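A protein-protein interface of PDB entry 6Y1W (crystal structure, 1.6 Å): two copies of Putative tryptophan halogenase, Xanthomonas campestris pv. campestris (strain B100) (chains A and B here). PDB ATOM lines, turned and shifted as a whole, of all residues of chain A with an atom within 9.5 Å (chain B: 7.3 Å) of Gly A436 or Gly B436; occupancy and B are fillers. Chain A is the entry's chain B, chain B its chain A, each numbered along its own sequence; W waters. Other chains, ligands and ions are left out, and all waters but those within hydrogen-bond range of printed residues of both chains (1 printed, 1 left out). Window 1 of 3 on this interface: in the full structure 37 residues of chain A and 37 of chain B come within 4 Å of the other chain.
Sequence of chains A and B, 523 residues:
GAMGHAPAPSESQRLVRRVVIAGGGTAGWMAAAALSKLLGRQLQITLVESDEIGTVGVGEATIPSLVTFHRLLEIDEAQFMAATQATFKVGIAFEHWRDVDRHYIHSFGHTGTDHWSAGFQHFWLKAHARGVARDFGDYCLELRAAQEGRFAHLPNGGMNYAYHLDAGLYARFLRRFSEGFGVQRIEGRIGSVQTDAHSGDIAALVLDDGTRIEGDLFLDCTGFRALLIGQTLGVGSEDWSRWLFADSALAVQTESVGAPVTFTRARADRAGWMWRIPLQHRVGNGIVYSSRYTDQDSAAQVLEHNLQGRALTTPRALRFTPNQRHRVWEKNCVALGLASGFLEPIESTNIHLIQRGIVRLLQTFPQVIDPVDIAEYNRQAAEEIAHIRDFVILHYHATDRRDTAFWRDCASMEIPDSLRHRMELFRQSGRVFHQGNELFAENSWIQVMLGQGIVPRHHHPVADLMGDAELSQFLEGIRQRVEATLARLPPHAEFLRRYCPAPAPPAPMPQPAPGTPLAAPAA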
ATOM      1  N   ARG A 356      19.943   6.759  -5.616  1.00  0.00           N
ATOM      2  CA  ARG A 356      21.081   7.654  -5.387  1.00  0.00           C
ATOM      3  C   ARG A 356      21.903   7.832  -6.653  1.00  0.00           C
ATOM      4  O   ARG A 356      22.368   8.942  -6.957  1.00  0.00           O
ATOM      5  CB  ARG A 356      21.988   7.141  -4.269  1.00  0.00           C
ATOM      6  CG  ARG A 356      21.427   7.246  -2.881  1.00  0.00           C
ATOM      7  CD  ARG A 356      21.172   8.708  -2.462  1.00  0.00           C
ATOM      8  NE  ARG A 356      22.402   9.466  -2.522  1.00  0.00           N
ATOM      9  CZ  ARG A 356      22.510  10.656  -3.105  1.00  0.00           C
ATOM     10  NH1 ARG A 356      21.445  11.240  -3.673  1.00  0.00           N
ATOM     11  NH2 ARG A 356      23.682  11.280  -3.109  1.00  0.00           N
ATOM     12  N   ARG A 379      33.673   9.564  -6.252  1.00  0.00           N
ATOM     13  CA  ARG A 379      34.065   9.746  -4.864  1.00  0.00           C
ATOM     14  C   ARG A 379      32.855   9.664  -3.948  1.00  0.00           C
ATOM     15  O   ARG A 379      32.899   8.995  -2.906  1.00  0.00           O
ATOM     16  CB  ARG A 379      34.797  11.083  -4.699  1.00  0.00           C
ATOM     17  CG  ARG A 379      35.290  11.364  -3.273  1.00  0.00           C
ATOM     18  CD  ARG A 379      35.658  12.838  -3.082  1.00  0.00           C
ATOM     19  NE  ARG A 379      34.499  13.730  -3.116  1.00  0.00           N
ATOM     20  CZ  ARG A 379      33.629  13.880  -2.121  1.00  0.00           C
ATOM     21  NH1 ARG A 379      33.782  13.187  -1.003  1.00  0.00           N
ATOM     22  NH2 ARG A 379      32.600  14.721  -2.241  1.00  0.00           N
ATOM     23  N   GLN A 380      31.767  10.328  -4.327  1.00  0.00           N
ATOM     24  CA  GLN A 380      30.561  10.282  -3.511  1.00  0.00           C
ATOM     25  C   GLN A 380      29.997   8.871  -3.460  1.00  0.00           C
ATOM     26  O   GLN A 380      29.623   8.386  -2.381  1.00  0.00           O
ATOM     27  CB  GLN A 380      29.499  11.236  -4.036  1.00  0.00           C
ATOM     28  CG  GLN A 380      29.838  12.700  -3.871  1.00  0.00           C
ATOM     29  CD  GLN A 380      28.681  13.605  -4.313  1.00  0.00           C
ATOM     30  OE1 GLN A 380      27.497  13.241  -4.201  1.00  0.00           O
ATOM     31  NE2 GLN A 380      29.025  14.782  -4.841  1.00  0.00           N
ATOM     32  N   GLU A 383      32.076   6.633  -1.122  1.00  0.00           N
ATOM     33  CA  GLU A 383      31.880   6.941   0.287  1.00  0.00           C
ATOM     34  C   GLU A 383      30.529   6.445   0.780  1.00  0.00           C
ATOM     35  O   GLU A 383      30.435   5.892   1.878  1.00  0.00           O
ATOM     36  CB  GLU A 383      31.996   8.451   0.513  1.00  0.00           C
ATOM     37  CG  GLU A 383      33.414   8.919   0.571  1.00  0.00           C
ATOM     38  CD  GLU A 383      33.553  10.428   0.486  1.00  0.00           C
ATOM     39  OE1 GLU A 383      32.528  11.148   0.518  1.00  0.00           O
ATOM     40  OE2 GLU A 383      34.706  10.893   0.387  1.00  0.00           O
ATOM     41  N   GLU A 384      29.475   6.643  -0.018  1.00  0.00           N
ATOM     42  CA  GLU A 384      28.141   6.252   0.418  1.00  0.00           C
ATOM     43  C   GLU A 384      28.049   4.747   0.573  1.00  0.00           C
ATOM     44  O   GLU A 384      27.468   4.265   1.545  1.00  0.00           O
ATOM     45  CB  GLU A 384      27.081   6.740  -0.577  1.00  0.00           C
ATOM     46  CG  GLU A 384      26.838   8.210  -0.448  1.00  0.00           C
ATOM     47  CD  GLU A 384      25.788   8.729  -1.434  1.00  0.00           C
ATOM     48  OE1 GLU A 384      24.746   8.061  -1.641  1.00  0.00           O
ATOM     49  OE2 GLU A 384      25.992   9.849  -1.927  1.00  0.00           O
ATOM     50  N   HIS A 387      29.870   3.123   3.673  1.00  0.00           N
ATOM     51  CA  HIS A 387      29.088   3.338   4.876  1.00  0.00           C
ATOM     52  C   HIS A 387      27.936   2.332   4.993  1.00  0.00           C
ATOM     53  O   HIS A 387      27.668   1.803   6.082  1.00  0.00           O
ATOM     54  CB  HIS A 387      28.539   4.760   4.881  1.00  0.00           C
ATOM     55  CG  HIS A 387      27.365   4.899   5.777  1.00  0.00           C
ATOM     56  ND1 HIS A 387      27.499   4.963   7.147  1.00  0.00           N
ATOM     57  CD2 HIS A 387      26.031   4.892   5.523  1.00  0.00           C
ATOM     58  CE1 HIS A 387      26.296   5.002   7.699  1.00  0.00           C
ATOM     59  NE2 HIS A 387      25.394   4.965   6.736  1.00  0.00           N
ATOM     60  N   ARG A 422      33.453   2.976  14.875  1.00  0.00           N
ATOM     61  CA  ARG A 422      32.100   3.360  15.315  1.00  0.00           C
ATOM     62  C   ARG A 422      31.616   2.466  16.455  1.00  0.00           C
ATOM     63  O   ARG A 422      30.984   2.940  17.415  1.00  0.00           O
ATOM     64  CB  ARG A 422      31.076   3.292  14.168  1.00  0.00           C
ATOM     65  CG  ARG A 422      31.468   3.906  12.856  1.00  0.00           C
ATOM     66  CD  ARG A 422      31.357   5.425  12.812  1.00  0.00           C
ATOM     67  NE  ARG A 422      29.992   5.960  12.750  1.00  0.00           N
ATOM     68  CZ  ARG A 422      29.442   6.557  11.691  1.00  0.00           C
ATOM     69  NH1 ARG A 422      30.098   6.699  10.543  1.00  0.00           N
ATOM     70  NH2 ARG A 422      28.213   7.022  11.784  1.00  0.00           N
ATOM     71  N   PHE A 433      27.868   9.362  15.694  1.00  0.00           N
ATOM     72  CA  PHE A 433      27.960  10.623  14.963  1.00  0.00           C
ATOM     73  C   PHE A 433      27.603  10.336  13.512  1.00  0.00           C
ATOM     74  O   PHE A 433      28.050   9.342  12.945  1.00  0.00           O
ATOM     75  CB  PHE A 433      29.363  11.268  15.044  1.00  0.00           C
ATOM     76  CG  PHE A 433      29.683  11.937  16.374  1.00  0.00           C
ATOM     77  CD1 PHE A 433      29.027  13.089  16.781  1.00  0.00           C
ATOM     78  CD2 PHE A 433      30.660  11.409  17.206  1.00  0.00           C
ATOM     79  CE1 PHE A 433      29.333  13.694  18.006  1.00  0.00           C
ATOM     80  CE2 PHE A 433      30.966  12.001  18.428  1.00  0.00           C
ATOM     81  CZ  PHE A 433      30.306  13.146  18.832  1.00  0.00           C
ATOM     82  N   HIS A 434      26.801  11.196  12.901  1.00  0.00           N
ATOM     83  CA  HIS A 434      26.467  10.996  11.503  1.00  0.00           C
ATOM     84  C   HIS A 434      27.245  11.976  10.628  1.00  0.00           C
ATOM     85  O   HIS A 434      27.355  13.152  10.955  1.00  0.00           O
ATOM     86  CB  HIS A 434      24.962  11.182  11.260  1.00  0.00           C
ATOM     87  CG  HIS A 434      24.587  11.349   9.815  1.00  0.00           C
ATOM     88  ND1 HIS A 434      24.674  12.563   9.162  1.00  0.00           N
ATOM     89  CD2 HIS A 434      24.084  10.472   8.911  1.00  0.00           C
ATOM     90  CE1 HIS A 434      24.274  12.416   7.910  1.00  0.00           C
ATOM     91  NE2 HIS A 434      23.918  11.155   7.730  1.00  0.00           N
ATOM     92  N   GLN A 435      27.806  11.473   9.523  1.00  0.00           N
ATOM     93  CA  GLN A 435      28.458  12.263   8.474  1.00  0.00           C
ATOM     94  C   GLN A 435      27.815  12.322   7.108  1.00  0.00           C
ATOM     95  O   GLN A 435      27.293  11.355   6.543  1.00  0.00           O
ATOM     96  CB  GLN A 435      29.963  12.039   8.168  1.00  0.00           C
ATOM     97  CG  GLN A 435      30.944  13.030   8.713  1.00  0.00           C
ATOM     98  CD  GLN A 435      32.409  12.674   8.440  1.00  0.00           C
ATOM     99  OE1 GLN A 435      32.779  11.497   8.111  1.00  0.00           O
ATOM    100  NE2 GLN A 435      33.100  13.784   8.033  1.00  0.00           N
ATOM    101  N   GLY A 436      27.902  13.562   6.643  1.00  0.00           N
ATOM    102  CA  GLY A 436      27.798  13.956   5.283  1.00  0.00           C
ATOM    103  C   GLY A 436      26.507  13.442   4.779  1.00  0.00           C
ATOM    104  O   GLY A 436      25.429  13.795   5.273  1.00  0.00           O
ATOM    105  N   ASN A 437      26.637  12.587   3.787  1.00  0.00           N
ATOM    106  CA  ASN A 437      25.497  11.969   3.176  1.00  0.00           C
ATOM    107  C   ASN A 437      25.428  10.483   3.493  1.00  0.00           C
ATOM    108  O   ASN A 437      24.885   9.720   2.698  1.00  0.00           O
ATOM    109  CB  ASN A 437      25.548  12.206   1.670  1.00  0.00           C
ATOM    110  CG  ASN A 437      24.194  12.497   1.085  1.00  0.00           C
ATOM    111  OD1 ASN A 437      23.254  12.834   1.817  1.00  0.00           O
ATOM    112  ND2 ASN A 437      24.063  12.333  -0.225  1.00  0.00           N
ATOM    113  N   GLU A 438      25.962  10.056   4.645  1.00  0.00           N
ATOM    114  CA  GLU A 438      25.735   8.677   5.079  1.00  0.00           C
ATOM    115  C   GLU A 438      24.245   8.404   5.189  1.00  0.00           C
ATOM    116  O   GLU A 438      23.479   9.224   5.706  1.00  0.00           O
ATOM    117  CB  GLU A 438      26.397   8.410   6.431  1.00  0.00           C
ATOM    118  CG  GLU A 438      27.918   8.403   6.357  1.00  0.00           C
ATOM    119  CD  GLU A 438      28.592   8.464   7.728  1.00  0.00           C
ATOM    120  OE1 GLU A 438      27.903   8.703   8.752  1.00  0.00           O
ATOM    121  OE2 GLU A 438      29.825   8.249   7.773  1.00  0.00           O
ATOM    122  N   LEU A 439      23.838   7.218   4.747  1.00  0.00           N
ATOM    123  CA  LEU A 439      22.424   6.862   4.818  1.00  0.00           C
ATOM    124  C   LEU A 439      21.950   6.714   6.265  1.00  0.00           C
ATOM    125  O   LEU A 439      20.934   7.307   6.659  1.00  0.00           O
ATOM    126  CB  LEU A 439      22.171   5.571   4.045  1.00  0.00           C
ATOM    127  CG  LEU A 439      20.796   4.977   4.271  1.00  0.00           C
ATOM    128  CD1 LEU A 439      19.724   5.977   3.778  1.00  0.00           C
ATOM    129  CD2 LEU A 439      20.737   3.687   3.473  1.00  0.00           C
ATOM    130  N   PHE A 440      22.657   5.928   7.084  1.00  0.00           N
ATOM    131  CA  PHE A 440      22.082   5.525   8.368  1.00  0.00           C
ATOM    132  C   PHE A 440      22.230   6.630   9.407  1.00  0.00           C
ATOM    133  O   PHE A 440      23.329   7.099   9.670  1.00  0.00           O
ATOM    134  CB  PHE A 440      22.710   4.205   8.834  1.00  0.00           C
ATOM    135  CG  PHE A 440      22.304   3.052   7.955  1.00  0.00           C
ATOM    136  CD1 PHE A 440      21.001   2.555   8.006  1.00  0.00           C
ATOM    137  CD2 PHE A 440      23.194   2.518   7.053  1.00  0.00           C
ATOM    138  CE1 PHE A 440      20.594   1.511   7.151  1.00  0.00           C
ATOM    139  CE2 PHE A 440      22.792   1.452   6.171  1.00  0.00           C
ATOM    140  CZ  PHE A 440      21.484   0.961   6.242  1.00  0.00           C
ATOM    141  N   ALA A 441      21.099   7.063   9.960  1.00  0.00           N
ATOM    142  CA  ALA A 441      21.065   8.127  10.952  1.00  0.00           C
ATOM    143  C   ALA A 441      21.549   7.630  12.317  1.00  0.00           C
ATOM    144  O   ALA A 441      21.720   6.431  12.550  1.00  0.00           O
ATOM    145  CB  ALA A 441      19.639   8.663  11.070  1.00  0.00           C
ATOM    146  N   PHE B 433      29.942  21.692  -4.153  1.00  0.00           N
ATOM    147  CA  PHE B 433      29.252  20.812  -3.222  1.00  0.00           C
ATOM    148  C   PHE B 433      29.649  21.197  -1.810  1.00  0.00           C
ATOM    149  O   PHE B 433      30.651  21.892  -1.587  1.00  0.00           O
ATOM    150  CB  PHE B 433      29.577  19.346  -3.490  1.00  0.00           C
ATOM    151  CG  PHE B 433      31.020  18.998  -3.276  1.00  0.00           C
ATOM    152  CD1 PHE B 433      31.943  19.125  -4.305  1.00  0.00           C
ATOM    153  CD2 PHE B 433      31.456  18.531  -2.032  1.00  0.00           C
ATOM    154  CE1 PHE B 433      33.263  18.785  -4.124  1.00  0.00           C
ATOM    155  CE2 PHE B 433      32.765  18.203  -1.828  1.00  0.00           C
ATOM    156  CZ  PHE B 433      33.685  18.330  -2.868  1.00  0.00           C
ATOM    157  N   HIS B 434      28.835  20.784  -0.854  1.00  0.00           N
ATOM    158  CA  HIS B 434      29.142  21.002   0.545  1.00  0.00           C
ATOM    159  C   HIS B 434      29.167  19.630   1.177  1.00  0.00           C
ATOM    160  O   HIS B 434      28.284  18.815   0.908  1.00  0.00           O
ATOM    161  CB  HIS B 434      28.108  21.889   1.248  1.00  0.00           C
ATOM    162  CG  HIS B 434      28.243  21.885   2.742  1.00  0.00           C
ATOM    163  ND1 HIS B 434      27.605  20.964   3.547  1.00  0.00           N
ATOM    164  CD2 HIS B 434      28.961  22.676   3.576  1.00  0.00           C
ATOM    165  CE1 HIS B 434      27.923  21.189   4.810  1.00  0.00           C
ATOM    166  NE2 HIS B 434      28.752  22.219   4.854  1.00  0.00           N
ATOM    167  N   GLN B 435      30.202  19.354   1.950  1.00  0.00           N
ATOM    168  CA  GLN B 435      30.343  18.042   2.578  1.00  0.00           C
ATOM    169  C   GLN B 435      30.369  18.177   4.095  1.00  0.00           C
ATOM    170  O   GLN B 435      31.000  19.089   4.626  1.00  0.00           O
ATOM    171  CB  GLN B 435      31.598  17.328   2.092  1.00  0.00           C
ATOM    172  CG  GLN B 435      31.870  16.023   2.834  1.00  0.00           C
ATOM    173  CD  GLN B 435      31.911  14.819   1.908  1.00  0.00           C
ATOM    174  OE1 GLN B 435      32.602  14.823   0.889  1.00  0.00           O
ATOM    175  NE2 GLN B 435      31.146  13.789   2.249  1.00  0.00           N
ATOM    176  N   GLY B 436      29.668  17.270   4.780  1.00  0.00           N
ATOM    177  CA  GLY B 436      29.731  17.103   6.219  1.00  0.00           C
ATOM    178  C   GLY B 436      29.468  18.353   7.033  1.00  0.00           C
ATOM    179  O   GLY B 436      28.428  18.998   6.867  1.00  0.00           O
ATOM    180  N   ASN B 437      30.406  18.708   7.915  1.00  0.00           N
ATOM    181  CA  ASN B 437      30.327  19.975   8.641  1.00  0.00           C
ATOM    182  C   ASN B 437      31.391  20.946   8.170  1.00  0.00           C
ATOM    183  O   ASN B 437      31.913  21.718   8.984  1.00  0.00           O
ATOM    184  CB  ASN B 437      30.457  19.866  10.175  1.00  0.00           C
ATOM    185  CG  ASN B 437      29.715  18.715  10.766  1.00  0.00           C
ATOM    186  OD1 ASN B 437      28.531  18.509  10.479  1.00  0.00           O
ATOM    187  ND2 ASN B 437      30.374  17.996  11.670  1.00  0.00           N
ATOM    188  N   GLU B 438      31.764  20.889   6.889  1.00  0.00           N
ATOM    189  CA  GLU B 438      32.593  21.963   6.355  1.00  0.00           C
ATOM    190  C   GLU B 438      31.915  23.290   6.655  1.00  0.00           C
ATOM    191  O   GLU B 438      30.687  23.413   6.565  1.00  0.00           O
ATOM    192  CB  GLU B 438      32.789  21.805   4.853  1.00  0.00           C
ATOM    193  CG  GLU B 438      33.742  20.699   4.512  1.00  0.00           C
ATOM    194  CD  GLU B 438      33.632  20.288   3.059  1.00  0.00           C
ATOM    195  OE1 GLU B 438      32.694  20.753   2.359  1.00  0.00           O
ATOM    196  OE2 GLU B 438      34.496  19.506   2.612  1.00  0.00           O
ATOM    197  N   LEU B 439      32.736  24.284   7.017  1.00  0.00           N
ATOM    198  CA  LEU B 439      32.190  25.599   7.327  1.00  0.00           C
ATOM    199  C   LEU B 439      31.565  26.253   6.098  1.00  0.00           C
ATOM    200  O   LEU B 439      30.472  26.812   6.180  1.00  0.00           O
ATOM    201  CB  LEU B 439      33.288  26.488   7.915  1.00  0.00           C
ATOM    202  CG  LEU B 439      32.911  27.962   8.032  1.00  0.00           C
ATOM    203  CD1 LEU B 439      31.726  28.183   8.987  1.00  0.00           C
ATOM    204  CD2 LEU B 439      34.124  28.743   8.518  1.00  0.00           C
HETATM  205  O   HOH W   1      29.279  10.924   2.752  1.00  0.00           O
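The guanidinium group of Arg A379 sits at hydrogen-bond distance from the side-chain amide oxygen of Gln B435 (2.8 Å). The side-chain amide nitrogen of Gln B435 sits at hydrogen-bond distance from the side-chain carboxylate of Glu A383 (3.4 Å).
The backbone NH (N) of Gln B435 sits at hydrogen-bond distance from the side-chain carboxylate (OE1) of Glu B438 (2.9 Å). The guanidinium group (NH1) of Arg A379 lies within salt-bridge range of the side-chain carboxylate (OE1) of Glu A383 (2.8 Å).
Arg A379 touches Phe B433. Gly B436 touches Gly A436.
Of chain B, only Gly B436 comes within 4 Å of Gly A436. Gly B436 touches just one residue of chain A: Gly A436. Of the printed residues of chain A, Gln B435 touches Arg A379 and Glu A383. Of the printed residues of chain B, Glu A383 touches Gln B435. The nearest residue of chain A that does not touch Gly B436 is Gln A435 (4.9 Å). The nearest printed residue of chain B that does not touch Glu A383 is Phe B433 (7.4 Å).
Of the 7 printed residues of chain B, 3 touch a printed residue of chain A.
Gly B436 touches its own counterpart, Gly A436. Positions printed for both chains: 433, 434, 435, 436, 437, 438 and 439. Of the 4 pairs that touch across the chains among the printed residues, 1 has its exchanged pair printed and touching as well.
Water W1 lies within hydrogen-bond range of the backbone NH (N) of Asn A437 (3.3 Å) and the side-chain amide nitrogen (NE2) of Gln B435 (3.5 Å).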
